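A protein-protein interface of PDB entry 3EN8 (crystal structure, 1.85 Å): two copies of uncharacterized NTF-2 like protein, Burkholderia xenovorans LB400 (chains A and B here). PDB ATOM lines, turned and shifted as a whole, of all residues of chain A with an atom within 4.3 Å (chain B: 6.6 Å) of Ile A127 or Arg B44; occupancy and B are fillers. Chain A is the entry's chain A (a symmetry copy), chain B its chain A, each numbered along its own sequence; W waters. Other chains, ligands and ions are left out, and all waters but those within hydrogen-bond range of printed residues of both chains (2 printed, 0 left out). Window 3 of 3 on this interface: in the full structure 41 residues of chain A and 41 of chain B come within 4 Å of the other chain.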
ATOM      1  N   ARG A  68       9.843 -14.843  27.183  1.00  0.00           N
ATOM      2  CA  ARG A  68      10.330 -13.456  27.314  1.00  0.00           C
ATOM      3  C   ARG A  68      10.128 -12.923  28.737  1.00  0.00           C
ATOM      4  O   ARG A  68      11.020 -12.399  29.428  1.00  0.00           O
ATOM      5  CB  ARG A  68       9.582 -12.531  26.343  1.00  0.00           C
ATOM      6  CG  ARG A  68      10.086 -11.097  26.395  1.00  0.00           C
ATOM      7  CD  ARG A  68       9.299 -10.136  25.503  1.00  0.00           C
ATOM      8  NE  ARG A  68       9.790  -8.748  25.589  1.00  0.00           N
ATOM      9  CZ  ARG A  68      10.726  -8.236  24.788  1.00  0.00           C
ATOM     10  NH1 ARG A  68      11.319  -8.981  23.870  1.00  0.00           N
ATOM     11  NH2 ARG A  68      11.105  -6.969  24.931  1.00  0.00           N
ATOM     12  N   VAL A 124      13.470   6.470  20.660  1.00  0.00           N
ATOM     13  CA  VAL A 124      13.331   5.155  21.261  1.00  0.00           C
ATOM     14  C   VAL A 124      14.665   4.505  21.589  1.00  0.00           C
ATOM     15  O   VAL A 124      15.692   4.741  20.962  1.00  0.00           O
ATOM     16  CB  VAL A 124      12.489   4.193  20.380  1.00  0.00           C
ATOM     17  CG1 VAL A 124      11.207   4.881  19.922  1.00  0.00           C
ATOM     18  CG2 VAL A 124      13.300   3.701  19.215  1.00  0.00           C
ATOM     19  N   GLN A 125      14.609   3.686  22.614  1.00  0.00           N
ATOM     20  CA  GLN A 125      15.694   2.800  22.954  1.00  0.00           C
ATOM     21  C   GLN A 125      15.408   1.429  22.363  1.00  0.00           C
ATOM     22  O   GLN A 125      14.284   0.924  22.405  1.00  0.00           O
ATOM     23  CB  GLN A 125      15.860   2.746  24.466  1.00  0.00           C
ATOM     24  CG  GLN A 125      17.037   1.951  24.924  1.00  0.00           C
ATOM     25  CD  GLN A 125      17.100   1.871  26.429  1.00  0.00           C
ATOM     26  OE1 GLN A 125      16.071   1.910  27.105  1.00  0.00           O
ATOM     27  NE2 GLN A 125      18.314   1.768  26.971  1.00  0.00           N
ATOM     28  N   GLN A 126      16.420   0.854  21.733  1.00  0.00           N
ATOM     29  CA  GLN A 126      16.295  -0.508  21.206  1.00  0.00           C
ATOM     30  C   GLN A 126      16.790  -1.481  22.256  1.00  0.00           C
ATOM     31  O   GLN A 126      17.985  -1.537  22.556  1.00  0.00           O
ATOM     32  CB  GLN A 126      17.067  -0.677  19.890  1.00  0.00           C
ATOM     33  CG  GLN A 126      17.207  -2.120  19.445  1.00  0.00           C
ATOM     34  CD  GLN A 126      15.903  -2.769  18.956  1.00  0.00           C
ATOM     35  OE1 GLN A 126      15.058  -2.138  18.275  1.00  0.00           O
ATOM     36  NE2 GLN A 126      15.755  -4.056  19.271  1.00  0.00           N
ATOM     37  N   ILE A 127      15.846  -2.231  22.815  1.00  0.00           N
ATOM     38  CA  ILE A 127      16.106  -3.115  23.966  1.00  0.00           C
ATOM     39  C   ILE A 127      16.028  -4.580  23.595  1.00  0.00           C
ATOM     40  O   ILE A 127      16.409  -5.452  24.365  1.00  0.00           O
ATOM     41  CB  ILE A 127      15.130  -2.861  25.141  1.00  0.00           C
ATOM     42  CG1 ILE A 127      13.683  -3.163  24.729  1.00  0.00           C
ATOM     43  CG2 ILE A 127      15.274  -1.424  25.652  1.00  0.00           C
ATOM     44  CD1 ILE A 127      12.723  -3.285  25.907  1.00  0.00           C
ATOM     45  N   GLY A 128      15.497  -4.836  22.414  1.00  0.00           N
ATOM     46  CA  GLY A 128      15.276  -6.201  21.955  1.00  0.00           C
ATOM     47  C   GLY A 128      14.041  -6.825  22.598  1.00  0.00           C
ATOM     48  O   GLY A 128      13.791  -8.016  22.416  1.00  0.00           O
ATOM     49  OXT GLY A 128      13.255  -6.177  23.311  1.00  0.00           O
ATOM     50  N   ILE B  35       7.527   3.767  31.071  1.00  0.00           N
ATOM     51  CA  ILE B  35       8.099   3.144  29.861  1.00  0.00           C
ATOM     52  C   ILE B  35       7.029   2.368  29.100  1.00  0.00           C
ATOM     53  O   ILE B  35       6.118   1.787  29.683  1.00  0.00           O
ATOM     54  CB  ILE B  35       9.350   2.261  30.162  1.00  0.00           C
ATOM     55  CG1 ILE B  35       9.023   1.114  31.119  1.00  0.00           C
ATOM     56  CG2 ILE B  35      10.445   3.155  30.779  1.00  0.00           C
ATOM     57  CD1 ILE B  35      10.133   0.028  31.314  1.00  0.00           C
ATOM     58  N   CYS B  36       7.167   2.404  27.781  1.00  0.00           N
ATOM     59  CA  CYS B  36       6.280   1.684  26.886  1.00  0.00           C
ATOM     60  C   CYS B  36       7.104   0.913  25.875  1.00  0.00           C
ATOM     61  O   CYS B  36       7.878   1.488  25.128  1.00  0.00           O
ATOM     62  CB  CYS B  36       5.316   2.620  26.168  1.00  0.00           C
ATOM     63  SG  CYS B  36       4.026   1.717  25.259  1.00  0.00           S
ATOM     64  N   ASP B  37       6.902  -0.396  25.895  1.00  0.00           N
ATOM     65  CA  ASP B  37       7.643  -1.363  25.053  1.00  0.00           C
ATOM     66  C   ASP B  37       6.771  -1.948  23.952  1.00  0.00           C
ATOM     67  O   ASP B  37       5.606  -2.301  24.164  1.00  0.00           O
ATOM     68  CB  ASP B  37       8.112  -2.537  25.906  1.00  0.00           C
ATOM     69  CG  ASP B  37       9.164  -2.172  26.923  1.00  0.00           C
ATOM     70  OD1 ASP B  37       9.751  -1.069  26.838  1.00  0.00           O
ATOM     71  OD2 ASP B  37       9.404  -3.014  27.832  1.00  0.00           O
ATOM     72  N   TYR B  38       7.374  -2.061  22.776  1.00  0.00           N
ATOM     73  CA  TYR B  38       6.840  -2.815  21.671  1.00  0.00           C
ATOM     74  C   TYR B  38       7.757  -4.010  21.405  1.00  0.00           C
ATOM     75  O   TYR B  38       8.728  -3.891  20.634  1.00  0.00           O
ATOM     76  CB  TYR B  38       6.775  -1.956  20.386  1.00  0.00           C
ATOM     77  CG  TYR B  38       6.072  -0.619  20.511  1.00  0.00           C
ATOM     78  CD1 TYR B  38       4.933  -0.463  21.309  1.00  0.00           C
ATOM     79  CD2 TYR B  38       6.510   0.477  19.797  1.00  0.00           C
ATOM     80  CE1 TYR B  38       4.280   0.740  21.399  1.00  0.00           C
ATOM     81  CE2 TYR B  38       5.857   1.695  19.880  1.00  0.00           C
ATOM     82  CZ  TYR B  38       4.743   1.824  20.689  1.00  0.00           C
ATOM     83  OH  TYR B  38       4.087   3.030  20.761  1.00  0.00           O
ATOM     84  N   SER B  41       9.083  -5.106  17.870  1.00  0.00           N
ATOM     85  CA  SER B  41      10.133  -4.306  17.212  1.00  0.00           C
ATOM     86  C   SER B  41      11.368  -4.043  18.078  1.00  0.00           C
ATOM     87  O   SER B  41      12.370  -3.540  17.589  1.00  0.00           O
ATOM     88  CB  SER B  41       9.551  -2.964  16.748  1.00  0.00           C
ATOM     89  OG  SER B  41       9.220  -2.196  17.902  1.00  0.00           O
ATOM     90  N   GLY B  42      11.283  -4.393  19.349  1.00  0.00           N
ATOM     91  CA  GLY B  42      12.381  -4.218  20.293  1.00  0.00           C
ATOM     92  C   GLY B  42      12.499  -2.790  20.784  1.00  0.00           C
ATOM     93  O   GLY B  42      13.499  -2.410  21.409  1.00  0.00           O
ATOM     94  N   GLU B  43      11.459  -2.004  20.520  1.00  0.00           N
ATOM     95  CA  GLU B  43      11.483  -0.571  20.855  1.00  0.00           C
ATOM     96  C   GLU B  43      10.985  -0.339  22.270  1.00  0.00           C
ATOM     97  O   GLU B  43      10.025  -0.978  22.729  1.00  0.00           O
ATOM     98  CB  GLU B  43      10.633   0.258  19.905  1.00  0.00           C
ATOM     99  CG  GLU B  43      11.110   0.246  18.506  1.00  0.00           C
ATOM    100  CD  GLU B  43      10.162   0.955  17.604  1.00  0.00           C
ATOM    101  OE1 GLU B  43       9.153   0.331  17.228  1.00  0.00           O
ATOM    102  OE2 GLU B  43      10.429   2.123  17.240  1.00  0.00           O
ATOM    103  N   ARG B  44      11.675   0.572  22.937  1.00  0.00           N
ATOM    104  CA  ARG B  44      11.237   1.090  24.214  1.00  0.00           C
ATOM    105  C   ARG B  44      11.141   2.625  24.217  1.00  0.00           C
ATOM    106  O   ARG B  44      12.062   3.326  23.815  1.00  0.00           O
ATOM    107  CB  ARG B  44      12.150   0.573  25.312  1.00  0.00           C
ATOM    108  CG  ARG B  44      11.971   1.293  26.617  1.00  0.00           C
ATOM    109  CD  ARG B  44      12.715   0.577  27.747  1.00  0.00           C
ATOM    110  NE  ARG B  44      12.076  -0.686  28.069  1.00  0.00           N
ATOM    111  CZ  ARG B  44      12.481  -1.533  28.999  1.00  0.00           C
ATOM    112  NH1 ARG B  44      13.551  -1.275  29.723  1.00  0.00           N
ATOM    113  NH2 ARG B  44      11.809  -2.651  29.195  1.00  0.00           N
ATOM    114  N   ILE B  45      10.014   3.134  24.699  1.00  0.00           N
ATOM    115  CA  ILE B  45       9.804   4.578  24.812  1.00  0.00           C
ATOM    116  C   ILE B  45       9.898   4.944  26.267  1.00  0.00           C
ATOM    117  O   ILE B  45       9.276   4.306  27.095  1.00  0.00           O
ATOM    118  CB  ILE B  45       8.423   4.997  24.237  1.00  0.00           C
ATOM    119  CG1 ILE B  45       8.356   4.677  22.743  1.00  0.00           C
ATOM    120  CG2 ILE B  45       8.125   6.490  24.490  1.00  0.00           C
ATOM    121  CD1 ILE B  45       6.966   4.707  22.143  1.00  0.00           C
ATOM    122  N   LEU B  46      10.706   5.965  26.574  1.00  0.00           N
ATOM    123  CA  LEU B  46      10.922   6.384  27.958  1.00  0.00           C
ATOM    124  C   LEU B  46      10.290   7.745  28.227  1.00  0.00           C
ATOM    125  O   LEU B  46      10.647   8.742  27.616  1.00  0.00           O
ATOM    126  CB  LEU B  46      12.436   6.415  28.260  1.00  0.00           C
ATOM    127  CG  LEU B  46      13.183   5.074  28.055  1.00  0.00           C
ATOM    128  CD1 LEU B  46      14.552   5.262  27.419  1.00  0.00           C
ATOM    129  CD2 LEU B  46      13.299   4.268  29.338  1.00  0.00           C
ATOM    130  N   HIS B 105       4.926   0.925  33.595  1.00  0.00           N
ATOM    131  CA  HIS B 105       5.384   0.102  32.459  1.00  0.00           C
ATOM    132  C   HIS B 105       4.186  -0.449  31.670  1.00  0.00           C
ATOM    133  O   HIS B 105       3.299  -1.099  32.200  1.00  0.00           O
ATOM    134  CB  HIS B 105       6.294  -1.025  32.966  1.00  0.00           C
ATOM    135  CG  HIS B 105       7.053  -1.772  31.892  1.00  0.00           C
ATOM    136  ND1 HIS B 105       8.028  -2.698  32.205  1.00  0.00           N
ATOM    137  CD2 HIS B 105       6.989  -1.740  30.539  1.00  0.00           C
ATOM    138  CE1 HIS B 105       8.546  -3.191  31.087  1.00  0.00           C
ATOM    139  NE2 HIS B 105       7.921  -2.641  30.060  1.00  0.00           N
HETATM  140  O   HOH W   1       9.658  -5.690  26.945  1.00  0.00           O
HETATM  141  O   HOH W   2      15.732   0.976  29.578  1.00  0.00           O
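OE2 of Glu B43 touches CG2 of Val A124, 3.8 Å away.
Val A124 touches Arg B44 (CA to O, 3.4 Å).
Gln A125 touches Gly B42.
CA of Glu B43 touches O of Gln A125, at 3.5 Å.
Leu B46 touches Gln A125 (CD1 to OE1, 3.7 Å).
O of Gly B42 touches CA of Gln A126 (3.4 Å).
Asp B37 touches Ile A127.
CD1 of Ile A127 touches NE of Arg B44, 3.4 Å away.
Water W2 lies within hydrogen-bond range of OE1 of Gln A125 (2.7 Å) and NH1 of Arg B44 (3.1 Å).
Water W1 bridges the guanidinium group (NH2) of Arg A68 and the side-chain carboxylate (OD2) of Asp B37.
The backbone carbonyl oxygen (O) of Ser B41 lies close to the side-chain amide oxygen (OE1) of Gln A126 (3.1 Å).
The backbone NH of Ile A127 lies within hydrogen-bond range of the backbone carbonyl oxygen of Gly B42, 2.7 Å away.
The backbone carbonyl oxygen (O) of Gly B42 lies within hydrogen-bond range of the backbone NH (N) of Gly A128.
The backbone NH (N) of Arg B44 sits at hydrogen-bond distance from the backbone carbonyl oxygen (O) of Gln A125.
No position is printed for both chains.
Of the 12 pairs that touch across the chains among the printed residues, none has its exchanged pair printed and touching as well.
Of the printed residues of chain A, Leu B46 touches Gln A125 (3.7 Å).
Printed residues of chain A within 4 Å of Glu B43: Val A124 and Gln A125.
Printed residues of chain B within 4 Å of Gln A126: Ser B41 (3.1 Å) and Gly B42 (3.4 Å).
His B105 touches none of the printed residues of chain A.
Cys B36 touches none of the printed residues of chain A.
The nearest residue of chain B that does not touch Ile A127 is Glu B43 (4.6 Å).
The nearest printed residue of chain A that does not touch Ser B41 is Gly A128 (5.9 Å).
OD1 of Asp B37 lies within salt-bridge range of NE of Arg B44 (2.7 Å).
OD2 of Asp B37 sits at hydrogen-bond distance from NE2 of His B105 (2.7 Å).
O of Tyr B38 lies within hydrogen-bond range of OG of Ser B41 (3.3 Å).
The backbone NH (N) of Tyr B38 is in hydrogen-bond range of the backbone carbonyl oxygen (O) of Glu B43, at 2.9 Å.
The chain-end carboxylate of Gly A128 is in salt-bridge range of the guanidinium group of Arg A68, 2.8 Å away.
The backbone NH (N) of Gly A128 sits close to the side-chain amide nitrogen (NE2) of Gln A126, at 3.2 Å.
Hydrophobic or aromatic side chains of chain B that line the printed part of chain A: Leu B46.
Of the 6 printed residues of chain A, 5 touch a printed residue of chain B.
Printed residues of chain A that touch a printed residue of chain B: Val A124, Gln A125, Gln A126, Ile A127 and Gly A128.
Hydrophobic or aromatic side chains of chain A within 4 Å of the printed part of chain B: Val A124 and Ile A127.
Along chain A the printed residues that touch a printed residue of chain B span positions 124 to 128.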
